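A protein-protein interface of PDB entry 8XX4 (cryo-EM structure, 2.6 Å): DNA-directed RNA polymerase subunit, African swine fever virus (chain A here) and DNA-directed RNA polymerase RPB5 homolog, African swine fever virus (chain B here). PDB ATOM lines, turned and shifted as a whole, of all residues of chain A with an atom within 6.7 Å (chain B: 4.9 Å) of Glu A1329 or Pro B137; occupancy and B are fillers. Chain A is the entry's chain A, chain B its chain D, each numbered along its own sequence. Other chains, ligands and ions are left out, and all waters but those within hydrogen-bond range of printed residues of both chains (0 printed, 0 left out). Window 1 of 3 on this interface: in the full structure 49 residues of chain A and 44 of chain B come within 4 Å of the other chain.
Of the 12 printed residues of chain B, 9 touch a printed residue of chain A.
Hydrophobic or aromatic side chains of chain B within 4 Å of the printed part of chain A: Ile B136, Pro B137, His B139, Ile B164 and Ile B184.
Hydrophobic or aromatic side chains of chain A that line the printed part of chain B: Tyr A1326, Ile A1328 and Ala A1330.
Among the printed residues, Asp or Glu carboxylates within 4 Å of a Lys or Arg side-chain nitrogen of the other chain: Glu A1329 with Arg B186, Glu A1329 with Arg B198 and Asp A1358 with Arg B186.
Of chain B, only Pro B137 (3.5 Å), His B139 (3.7 Å), Ile B184 (3.4 Å), Arg B186 (2.7 Å) and Arg B198 (2.7 Å) come within 4 Å of Glu A1329.
Pro B137 touches just one residue of chain A: Glu A1329.
Printed residues of chain A within 4 Å of Ala B135: Ala A1330 (3.4 Å).
Of the printed residues of chain B, Gln A1333 touches Pro B187.
Of the printed residues of chain A, Ile B136 touches Tyr A1326.
Printed residues of chain A within 4 Å of Ile B164: Ile A1328 (3.7 Å).
Of the printed residues of chain A, Arg B198 touches Ile A1328, Glu A1329 and Thr A1361.
Val B196 touches none of the printed residues of chain A.
Met A1323 touches none of the printed residues of chain B.
The nearest residue of chain B that does not touch Glu A1329 is Val B196 (4.4 Å).
The nearest residue of chain A that does not touch Pro B137 is Ala A1330 (4.3 Å).
O of Thr A1361 sits close to NH2 of Arg B198, 2.4 Å away.
The side-chain carboxylate (OE2) of Glu A1329 lies within salt-bridge range of the guanidinium group (NH1) of Arg B198, at 2.7 Å.
The side-chain carboxylate (OE2) of Glu A1329 is in salt-bridge range of the guanidinium group (NH2) of Arg B186, 2.7 Å away.
The backbone carbonyl oxygen (O) of Pro B187 sits at hydrogen-bond distance from the side-chain amide nitrogen (NE2) of Gln A1333, at 3.0 Å.
The guanidinium group of Arg A1332 lies close to the guanidinium group of Arg B186, at 3.4 Å.
NH1 of Arg B186 lies within salt-bridge range of OD1 of Asp A1358 (3.2 Å).
A ring nitrogen (ND1) of His B139 sits at hydrogen-bond distance from the backbone carbonyl oxygen of Pro B137 (2.7 Å).
NH1 of Arg A1332 sits close to NE2 of Gln A1333 (3.2 Å).
The backbone carbonyl oxygen (O) of Val B196 lies within hydrogen-bond range of the backbone NH (N) of Ile B184 (2.7 Å).
The guanidinium group (NE) of Arg A1332 is in salt-bridge range of the side-chain carboxylate (OD1) of Asp A1358.
Among the printed residues, merely in contact across the chains: Ala A1330 with Ala B135 (3.4 Å), Glu A1329 with Ile B184 (3.4 Å), Tyr A1326 with Ile B136 (3.5 Å), Glu A1329 with Pro B137 (3.5 Å), Ile A1328 with Ile B164 (3.7 Å), Glu A1329 with His B139 (3.7 Å) and Ile A1328 with Arg B198 (3.8 Å).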
ATOM      1  N   ASN A 914     -20.999  32.531  26.588  1.00  0.00           N
ATOM      2  CA  ASN A 914     -21.040  31.136  26.162  1.00  0.00           C
ATOM      3  C   ASN A 914     -19.634  30.594  25.921  1.00  0.00           C
ATOM      4  O   ASN A 914     -19.314  29.463  26.316  1.00  0.00           O
ATOM      5  CB  ASN A 914     -21.896  31.006  24.905  1.00  0.00           C
ATOM      6  CG  ASN A 914     -22.177  29.572  24.540  1.00  0.00           C
ATOM      7  OD1 ASN A 914     -21.511  28.997  23.686  1.00  0.00           O
ATOM      8  ND2 ASN A 914     -23.168  28.984  25.189  1.00  0.00           N
ATOM      9  N   MET A1323     -16.282  15.146  20.790  1.00  0.00           N
ATOM     10  CA  MET A1323     -16.832  14.798  19.487  1.00  0.00           C
ATOM     11  C   MET A1323     -17.909  13.730  19.605  1.00  0.00           C
ATOM     12  O   MET A1323     -18.957  13.823  18.958  1.00  0.00           O
ATOM     13  CB  MET A1323     -15.712  14.334  18.559  1.00  0.00           C
ATOM     14  CG  MET A1323     -16.201  13.618  17.327  1.00  0.00           C
ATOM     15  SD  MET A1323     -16.976  14.735  16.160  1.00  0.00           S
ATOM     16  CE  MET A1323     -17.581  13.578  14.947  1.00  0.00           C
ATOM     17  N   TYR A1326     -20.959  15.529  21.702  1.00  0.00           N
ATOM     18  CA  TYR A1326     -21.522  16.818  21.320  1.00  0.00           C
ATOM     19  C   TYR A1326     -21.594  17.052  19.822  1.00  0.00           C
ATOM     20  O   TYR A1326     -22.533  17.694  19.355  1.00  0.00           O
ATOM     21  CB  TYR A1326     -20.719  17.947  21.968  1.00  0.00           C
ATOM     22  CG  TYR A1326     -20.834  18.000  23.472  1.00  0.00           C
ATOM     23  CD1 TYR A1326     -21.949  17.497  24.120  1.00  0.00           C
ATOM     24  CD2 TYR A1326     -19.826  18.552  24.241  1.00  0.00           C
ATOM     25  CE1 TYR A1326     -22.057  17.540  25.490  1.00  0.00           C
ATOM     26  CE2 TYR A1326     -19.925  18.601  25.614  1.00  0.00           C
ATOM     27  CZ  TYR A1326     -21.043  18.095  26.232  1.00  0.00           C
ATOM     28  OH  TYR A1326     -21.145  18.146  27.599  1.00  0.00           O
ATOM     29  N   GLY A1327     -20.635  16.566  19.045  1.00  0.00           N
ATOM     30  CA  GLY A1327     -20.684  16.720  17.610  1.00  0.00           C
ATOM     31  C   GLY A1327     -19.380  17.250  17.072  1.00  0.00           C
ATOM     32  O   GLY A1327     -18.369  17.318  17.773  1.00  0.00           O
ATOM     33  N   ILE A1328     -19.400  17.644  15.800  1.00  0.00           N
ATOM     34  CA  ILE A1328     -18.172  18.078  15.149  1.00  0.00           C
ATOM     35  C   ILE A1328     -17.895  19.553  15.407  1.00  0.00           C
ATOM     36  O   ILE A1328     -16.736  19.972  15.422  1.00  0.00           O
ATOM     37  CB  ILE A1328     -18.226  17.767  13.642  1.00  0.00           C
ATOM     38  CG1 ILE A1328     -16.839  17.892  13.024  1.00  0.00           C
ATOM     39  CG2 ILE A1328     -19.203  18.675  12.927  1.00  0.00           C
ATOM     40  CD1 ILE A1328     -15.797  17.069  13.714  1.00  0.00           C
ATOM     41  N   GLU A1329     -18.930  20.363  15.622  1.00  0.00           N
ATOM     42  CA  GLU A1329     -18.706  21.780  15.884  1.00  0.00           C
ATOM     43  C   GLU A1329     -18.146  22.000  17.281  1.00  0.00           C
ATOM     44  O   GLU A1329     -17.205  22.784  17.470  1.00  0.00           O
ATOM     45  CB  GLU A1329     -20.009  22.545  15.692  1.00  0.00           C
ATOM     46  CG  GLU A1329     -20.517  22.498  14.279  1.00  0.00           C
ATOM     47  CD  GLU A1329     -19.704  23.368  13.354  1.00  0.00           C
ATOM     48  OE1 GLU A1329     -19.346  24.491  13.757  1.00  0.00           O
ATOM     49  OE2 GLU A1329     -19.406  22.925  12.230  1.00  0.00           O
ATOM     50  N   ALA A1330     -18.709  21.312  18.272  1.00  0.00           N
ATOM     51  CA  ALA A1330     -18.133  21.353  19.605  1.00  0.00           C
ATOM     52  C   ALA A1330     -16.737  20.755  19.621  1.00  0.00           C
ATOM     53  O   ALA A1330     -15.872  21.229  20.360  1.00  0.00           O
ATOM     54  CB  ALA A1330     -19.041  20.625  20.588  1.00  0.00           C
ATOM     55  N   ALA A1331     -16.491  19.725  18.809  1.00  0.00           N
ATOM     56  CA  ALA A1331     -15.152  19.152  18.729  1.00  0.00           C
ATOM     57  C   ALA A1331     -14.166  20.126  18.100  1.00  0.00           C
ATOM     58  O   ALA A1331     -12.999  20.178  18.495  1.00  0.00           O
ATOM     59  CB  ALA A1331     -15.181  17.845  17.945  1.00  0.00           C
ATOM     60  N   ARG A1332     -14.609  20.900  17.111  1.00  0.00           N
ATOM     61  CA  ARG A1332     -13.740  21.910  16.519  1.00  0.00           C
ATOM     62  C   ARG A1332     -13.421  23.014  17.519  1.00  0.00           C
ATOM     63  O   ARG A1332     -12.274  23.475  17.607  1.00  0.00           O
ATOM     64  CB  ARG A1332     -14.393  22.482  15.265  1.00  0.00           C
ATOM     65  CG  ARG A1332     -13.776  23.766  14.781  1.00  0.00           C
ATOM     66  CD  ARG A1332     -14.643  24.430  13.742  1.00  0.00           C
ATOM     67  NE  ARG A1332     -14.226  25.806  13.507  1.00  0.00           N
ATOM     68  CZ  ARG A1332     -14.515  26.820  14.309  1.00  0.00           C
ATOM     69  NH1 ARG A1332     -15.234  26.651  15.404  1.00  0.00           N
ATOM     70  NH2 ARG A1332     -14.075  28.035  14.002  1.00  0.00           N
ATOM     71  N   GLN A1333     -14.419  23.446  18.291  1.00  0.00           N
ATOM     72  CA  GLN A1333     -14.152  24.410  19.352  1.00  0.00           C
ATOM     73  C   GLN A1333     -13.205  23.830  20.395  1.00  0.00           C
ATOM     74  O   GLN A1333     -12.343  24.538  20.930  1.00  0.00           O
ATOM     75  CB  GLN A1333     -15.459  24.856  20.000  1.00  0.00           C
ATOM     76  CG  GLN A1333     -16.318  25.726  19.116  1.00  0.00           C
ATOM     77  CD  GLN A1333     -15.786  27.135  18.990  1.00  0.00           C
ATOM     78  OE1 GLN A1333     -14.833  27.513  19.663  1.00  0.00           O
ATOM     79  NE2 GLN A1333     -16.406  27.922  18.125  1.00  0.00           N
ATOM     80  N   LYS A1334     -13.350  22.540  20.697  1.00  0.00           N
ATOM     81  CA  LYS A1334     -12.446  21.884  21.632  1.00  0.00           C
ATOM     82  C   LYS A1334     -11.028  21.846  21.091  1.00  0.00           C
ATOM     83  O   LYS A1334     -10.066  22.013  21.845  1.00  0.00           O
ATOM     84  CB  LYS A1334     -12.945  20.473  21.936  1.00  0.00           C
ATOM     85  CG  LYS A1334     -12.275  19.812  23.118  1.00  0.00           C
ATOM     86  CD  LYS A1334     -12.243  20.727  24.318  1.00  0.00           C
ATOM     87  CE  LYS A1334     -13.631  20.977  24.865  1.00  0.00           C
ATOM     88  NZ  LYS A1334     -13.582  21.847  26.060  1.00  0.00           N
ATOM     89  N   ILE A1336      -9.718  24.041  19.021  1.00  0.00           N
ATOM     90  CA  ILE A1336      -9.224  25.407  19.188  1.00  0.00           C
ATOM     91  C   ILE A1336      -8.750  25.628  20.619  1.00  0.00           C
ATOM     92  O   ILE A1336      -7.645  26.127  20.856  1.00  0.00           O
ATOM     93  CB  ILE A1336     -10.308  26.426  18.801  1.00  0.00           C
ATOM     94  CG1 ILE A1336     -10.510  26.462  17.293  1.00  0.00           C
ATOM     95  CG2 ILE A1336      -9.936  27.801  19.297  1.00  0.00           C
ATOM     96  CD1 ILE A1336     -11.937  26.697  16.891  1.00  0.00           C
ATOM     97  N   ASP A1358     -10.443  23.823  11.681  1.00  0.00           N
ATOM     98  CA  ASP A1358     -11.319  23.646  10.533  1.00  0.00           C
ATOM     99  C   ASP A1358     -10.751  22.643   9.545  1.00  0.00           C
ATOM    100  O   ASP A1358     -11.513  21.934   8.881  1.00  0.00           O
ATOM    101  CB  ASP A1358     -11.562  24.989   9.850  1.00  0.00           C
ATOM    102  CG  ASP A1358     -12.719  25.749  10.458  1.00  0.00           C
ATOM    103  OD1 ASP A1358     -13.807  25.161  10.600  1.00  0.00           O
ATOM    104  OD2 ASP A1358     -12.544  26.934  10.799  1.00  0.00           O
ATOM    105  N   THR A1361     -11.589  19.128  11.025  1.00  0.00           N
ATOM    106  CA  THR A1361     -12.995  18.784  11.205  1.00  0.00           C
ATOM    107  C   THR A1361     -13.814  18.994   9.939  1.00  0.00           C
ATOM    108  O   THR A1361     -15.044  18.966   9.996  1.00  0.00           O
ATOM    109  CB  THR A1361     -13.603  19.584  12.358  1.00  0.00           C
ATOM    110  OG1 THR A1361     -13.551  20.980  12.055  1.00  0.00           O
ATOM    111  CG2 THR A1361     -12.854  19.324  13.647  1.00  0.00           C
ATOM    112  N   ALA B 135     -21.572  24.053  24.746  1.00  0.00           N
ATOM    113  CA  ALA B 135     -20.511  23.824  23.773  1.00  0.00           C
ATOM    114  C   ALA B 135     -21.026  23.616  22.359  1.00  0.00           C
ATOM    115  O   ALA B 135     -20.232  23.694  21.418  1.00  0.00           O
ATOM    116  CB  ALA B 135     -19.673  22.617  24.190  1.00  0.00           C
ATOM    117  N   ILE B 136     -22.314  23.359  22.185  1.00  0.00           N
ATOM    118  CA  ILE B 136     -22.894  23.048  20.883  1.00  0.00           C
ATOM    119  C   ILE B 136     -23.468  24.334  20.299  1.00  0.00           C
ATOM    120  O   ILE B 136     -24.393  24.907  20.892  1.00  0.00           O
ATOM    121  CB  ILE B 136     -23.976  21.966  20.994  1.00  0.00           C
ATOM    122  CG1 ILE B 136     -23.352  20.631  21.382  1.00  0.00           C
ATOM    123  CG2 ILE B 136     -24.731  21.839  19.695  1.00  0.00           C
ATOM    124  CD1 ILE B 136     -24.358  19.556  21.667  1.00  0.00           C
ATOM    125  N   PRO B 137     -22.967  24.817  19.166  1.00  0.00           N
ATOM    126  CA  PRO B 137     -23.566  25.995  18.538  1.00  0.00           C
ATOM    127  C   PRO B 137     -24.926  25.670  17.946  1.00  0.00           C
ATOM    128  O   PRO B 137     -25.299  24.510  17.770  1.00  0.00           O
ATOM    129  CB  PRO B 137     -22.560  26.369  17.449  1.00  0.00           C
ATOM    130  CG  PRO B 137     -21.848  25.118  17.160  1.00  0.00           C
ATOM    131  CD  PRO B 137     -21.789  24.338  18.428  1.00  0.00           C
ATOM    132  N   LYS B 138     -25.673  26.721  17.638  1.00  0.00           N
ATOM    133  CA  LYS B 138     -27.056  26.555  17.211  1.00  0.00           C
ATOM    134  C   LYS B 138     -27.098  26.014  15.789  1.00  0.00           C
ATOM    135  O   LYS B 138     -26.778  26.724  14.832  1.00  0.00           O
ATOM    136  CB  LYS B 138     -27.808  27.877  17.321  1.00  0.00           C
ATOM    137  CG  LYS B 138     -28.686  27.978  18.560  1.00  0.00           C
ATOM    138  CD  LYS B 138     -27.977  27.427  19.790  1.00  0.00           C
ATOM    139  CE  LYS B 138     -28.739  27.724  21.068  1.00  0.00           C
ATOM    140  NZ  LYS B 138     -29.860  26.775  21.284  1.00  0.00           N
ATOM    141  N   HIS B 139     -27.485  24.751  15.655  1.00  0.00           N
ATOM    142  CA  HIS B 139     -27.714  24.146  14.357  1.00  0.00           C
ATOM    143  C   HIS B 139     -29.140  24.415  13.905  1.00  0.00           C
ATOM    144  O   HIS B 139     -30.062  24.519  14.718  1.00  0.00           O
ATOM    145  CB  HIS B 139     -27.477  22.639  14.414  1.00  0.00           C
ATOM    146  CG  HIS B 139     -26.057  22.253  14.673  1.00  0.00           C
ATOM    147  ND1 HIS B 139     -25.305  22.810  15.682  1.00  0.00           N
ATOM    148  CD2 HIS B 139     -25.256  21.349  14.062  1.00  0.00           C
ATOM    149  CE1 HIS B 139     -24.098  22.275  15.675  1.00  0.00           C
ATOM    150  NE2 HIS B 139     -24.044  21.385  14.703  1.00  0.00           N
ATOM    151  N   ILE B 164     -21.195  17.063   7.610  1.00  0.00           N
ATOM    152  CA  ILE B 164     -21.616  16.736   8.963  1.00  0.00           C
ATOM    153  C   ILE B 164     -22.354  15.407   8.910  1.00  0.00           C
ATOM    154  O   ILE B 164     -23.136  15.155   7.986  1.00  0.00           O
ATOM    155  CB  ILE B 164     -22.483  17.855   9.581  1.00  0.00           C
ATOM    156  CG1 ILE B 164     -22.628  17.657  11.086  1.00  0.00           C
ATOM    157  CG2 ILE B 164     -23.842  17.941   8.923  1.00  0.00           C
ATOM    158  CD1 ILE B 164     -22.752  18.943  11.840  1.00  0.00           C
ATOM    159  N   ILE B 184     -25.065  26.613  10.733  1.00  0.00           N
ATOM    160  CA  ILE B 184     -24.511  26.610  12.079  1.00  0.00           C
ATOM    161  C   ILE B 184     -24.038  28.014  12.416  1.00  0.00           C
ATOM    162  O   ILE B 184     -23.313  28.635  11.634  1.00  0.00           O
ATOM    163  CB  ILE B 184     -23.365  25.592  12.208  1.00  0.00           C
ATOM    164  CG1 ILE B 184     -23.792  24.267  11.578  1.00  0.00           C
ATOM    165  CG2 ILE B 184     -22.985  25.410  13.658  1.00  0.00           C
ATOM    166  CD1 ILE B 184     -22.778  23.187  11.659  1.00  0.00           C
ATOM    167  N   GLU B 185     -24.460  28.512  13.575  1.00  0.00           N
ATOM    168  CA  GLU B 185     -24.048  29.817  14.089  1.00  0.00           C
ATOM    169  C   GLU B 185     -22.963  29.574  15.128  1.00  0.00           C
ATOM    170  O   GLU B 185     -23.241  29.414  16.315  1.00  0.00           O
ATOM    171  CB  GLU B 185     -25.232  30.562  14.689  1.00  0.00           C
ATOM    172  CG  GLU B 185     -25.911  31.528  13.750  1.00  0.00           C
ATOM    173  CD  GLU B 185     -25.367  32.932  13.882  1.00  0.00           C
ATOM    174  OE1 GLU B 185     -24.283  33.092  14.477  1.00  0.00           O
ATOM    175  OE2 GLU B 185     -26.025  33.877  13.400  1.00  0.00           O
ATOM    176  N   ARG B 186     -21.716  29.543  14.675  1.00  0.00           N
ATOM    177  CA  ARG B 186     -20.698  29.218  15.663  1.00  0.00           C
ATOM    178  C   ARG B 186     -20.102  30.487  16.257  1.00  0.00           C
ATOM    179  O   ARG B 186     -19.853  31.449  15.530  1.00  0.00           O
ATOM    180  CB  ARG B 186     -19.589  28.380  15.041  1.00  0.00           C
ATOM    181  CG  ARG B 186     -19.239  28.778  13.631  1.00  0.00           C
ATOM    182  CD  ARG B 186     -17.964  28.107  13.164  1.00  0.00           C
ATOM    183  NE  ARG B 186     -18.215  26.769  12.647  1.00  0.00           N
ATOM    184  CZ  ARG B 186     -17.484  26.179  11.712  1.00  0.00           C
ATOM    185  NH1 ARG B 186     -16.452  26.787  11.156  1.00  0.00           N
ATOM    186  NH2 ARG B 186     -17.803  24.950  11.320  1.00  0.00           N
ATOM    187  N   PRO B 187     -19.875  30.515  17.569  1.00  0.00           N
ATOM    188  CA  PRO B 187     -19.174  31.654  18.167  1.00  0.00           C
ATOM    189  C   PRO B 187     -17.756  31.760  17.633  1.00  0.00           C
ATOM    190  O   PRO B 187     -17.079  30.760  17.394  1.00  0.00           O
ATOM    191  CB  PRO B 187     -19.184  31.340  19.667  1.00  0.00           C
ATOM    192  CG  PRO B 187     -20.146  30.229  19.844  1.00  0.00           C
ATOM    193  CD  PRO B 187     -20.213  29.486  18.561  1.00  0.00           C
ATOM    194  N   VAL B 196     -21.903  29.135   9.197  1.00  0.00           N
ATOM    195  CA  VAL B 196     -21.371  28.123   8.298  1.00  0.00           C
ATOM    196  C   VAL B 196     -22.503  27.184   7.909  1.00  0.00           C
ATOM    197  O   VAL B 196     -23.476  27.015   8.649  1.00  0.00           O
ATOM    198  CB  VAL B 196     -20.197  27.360   8.954  1.00  0.00           C
ATOM    199  CG1 VAL B 196     -20.576  25.926   9.282  1.00  0.00           C
ATOM    200  CG2 VAL B 196     -18.979  27.413   8.071  1.00  0.00           C
ATOM    201  N   ARG B 198     -23.167  23.243   6.468  1.00  0.00           N
ATOM    202  CA  ARG B 198     -22.549  21.936   6.332  1.00  0.00           C
ATOM    203  C   ARG B 198     -23.499  20.973   5.640  1.00  0.00           C
ATOM    204  O   ARG B 198     -24.713  21.017   5.844  1.00  0.00           O
ATOM    205  CB  ARG B 198     -22.137  21.372   7.690  1.00  0.00           C
ATOM    206  CG  ARG B 198     -20.933  22.050   8.291  1.00  0.00           C
ATOM    207  CD  ARG B 198     -20.491  21.356   9.553  1.00  0.00           C
ATOM    208  NE  ARG B 198     -19.416  20.407   9.309  1.00  0.00           N
ATOM    209  CZ  ARG B 198     -18.193  20.519   9.805  1.00  0.00           C
ATOM    210  NH1 ARG B 198     -17.853  21.535  10.576  1.00  0.00           N
ATOM    211  NH2 ARG B 198     -17.291  19.589   9.518  1.00  0.00           N
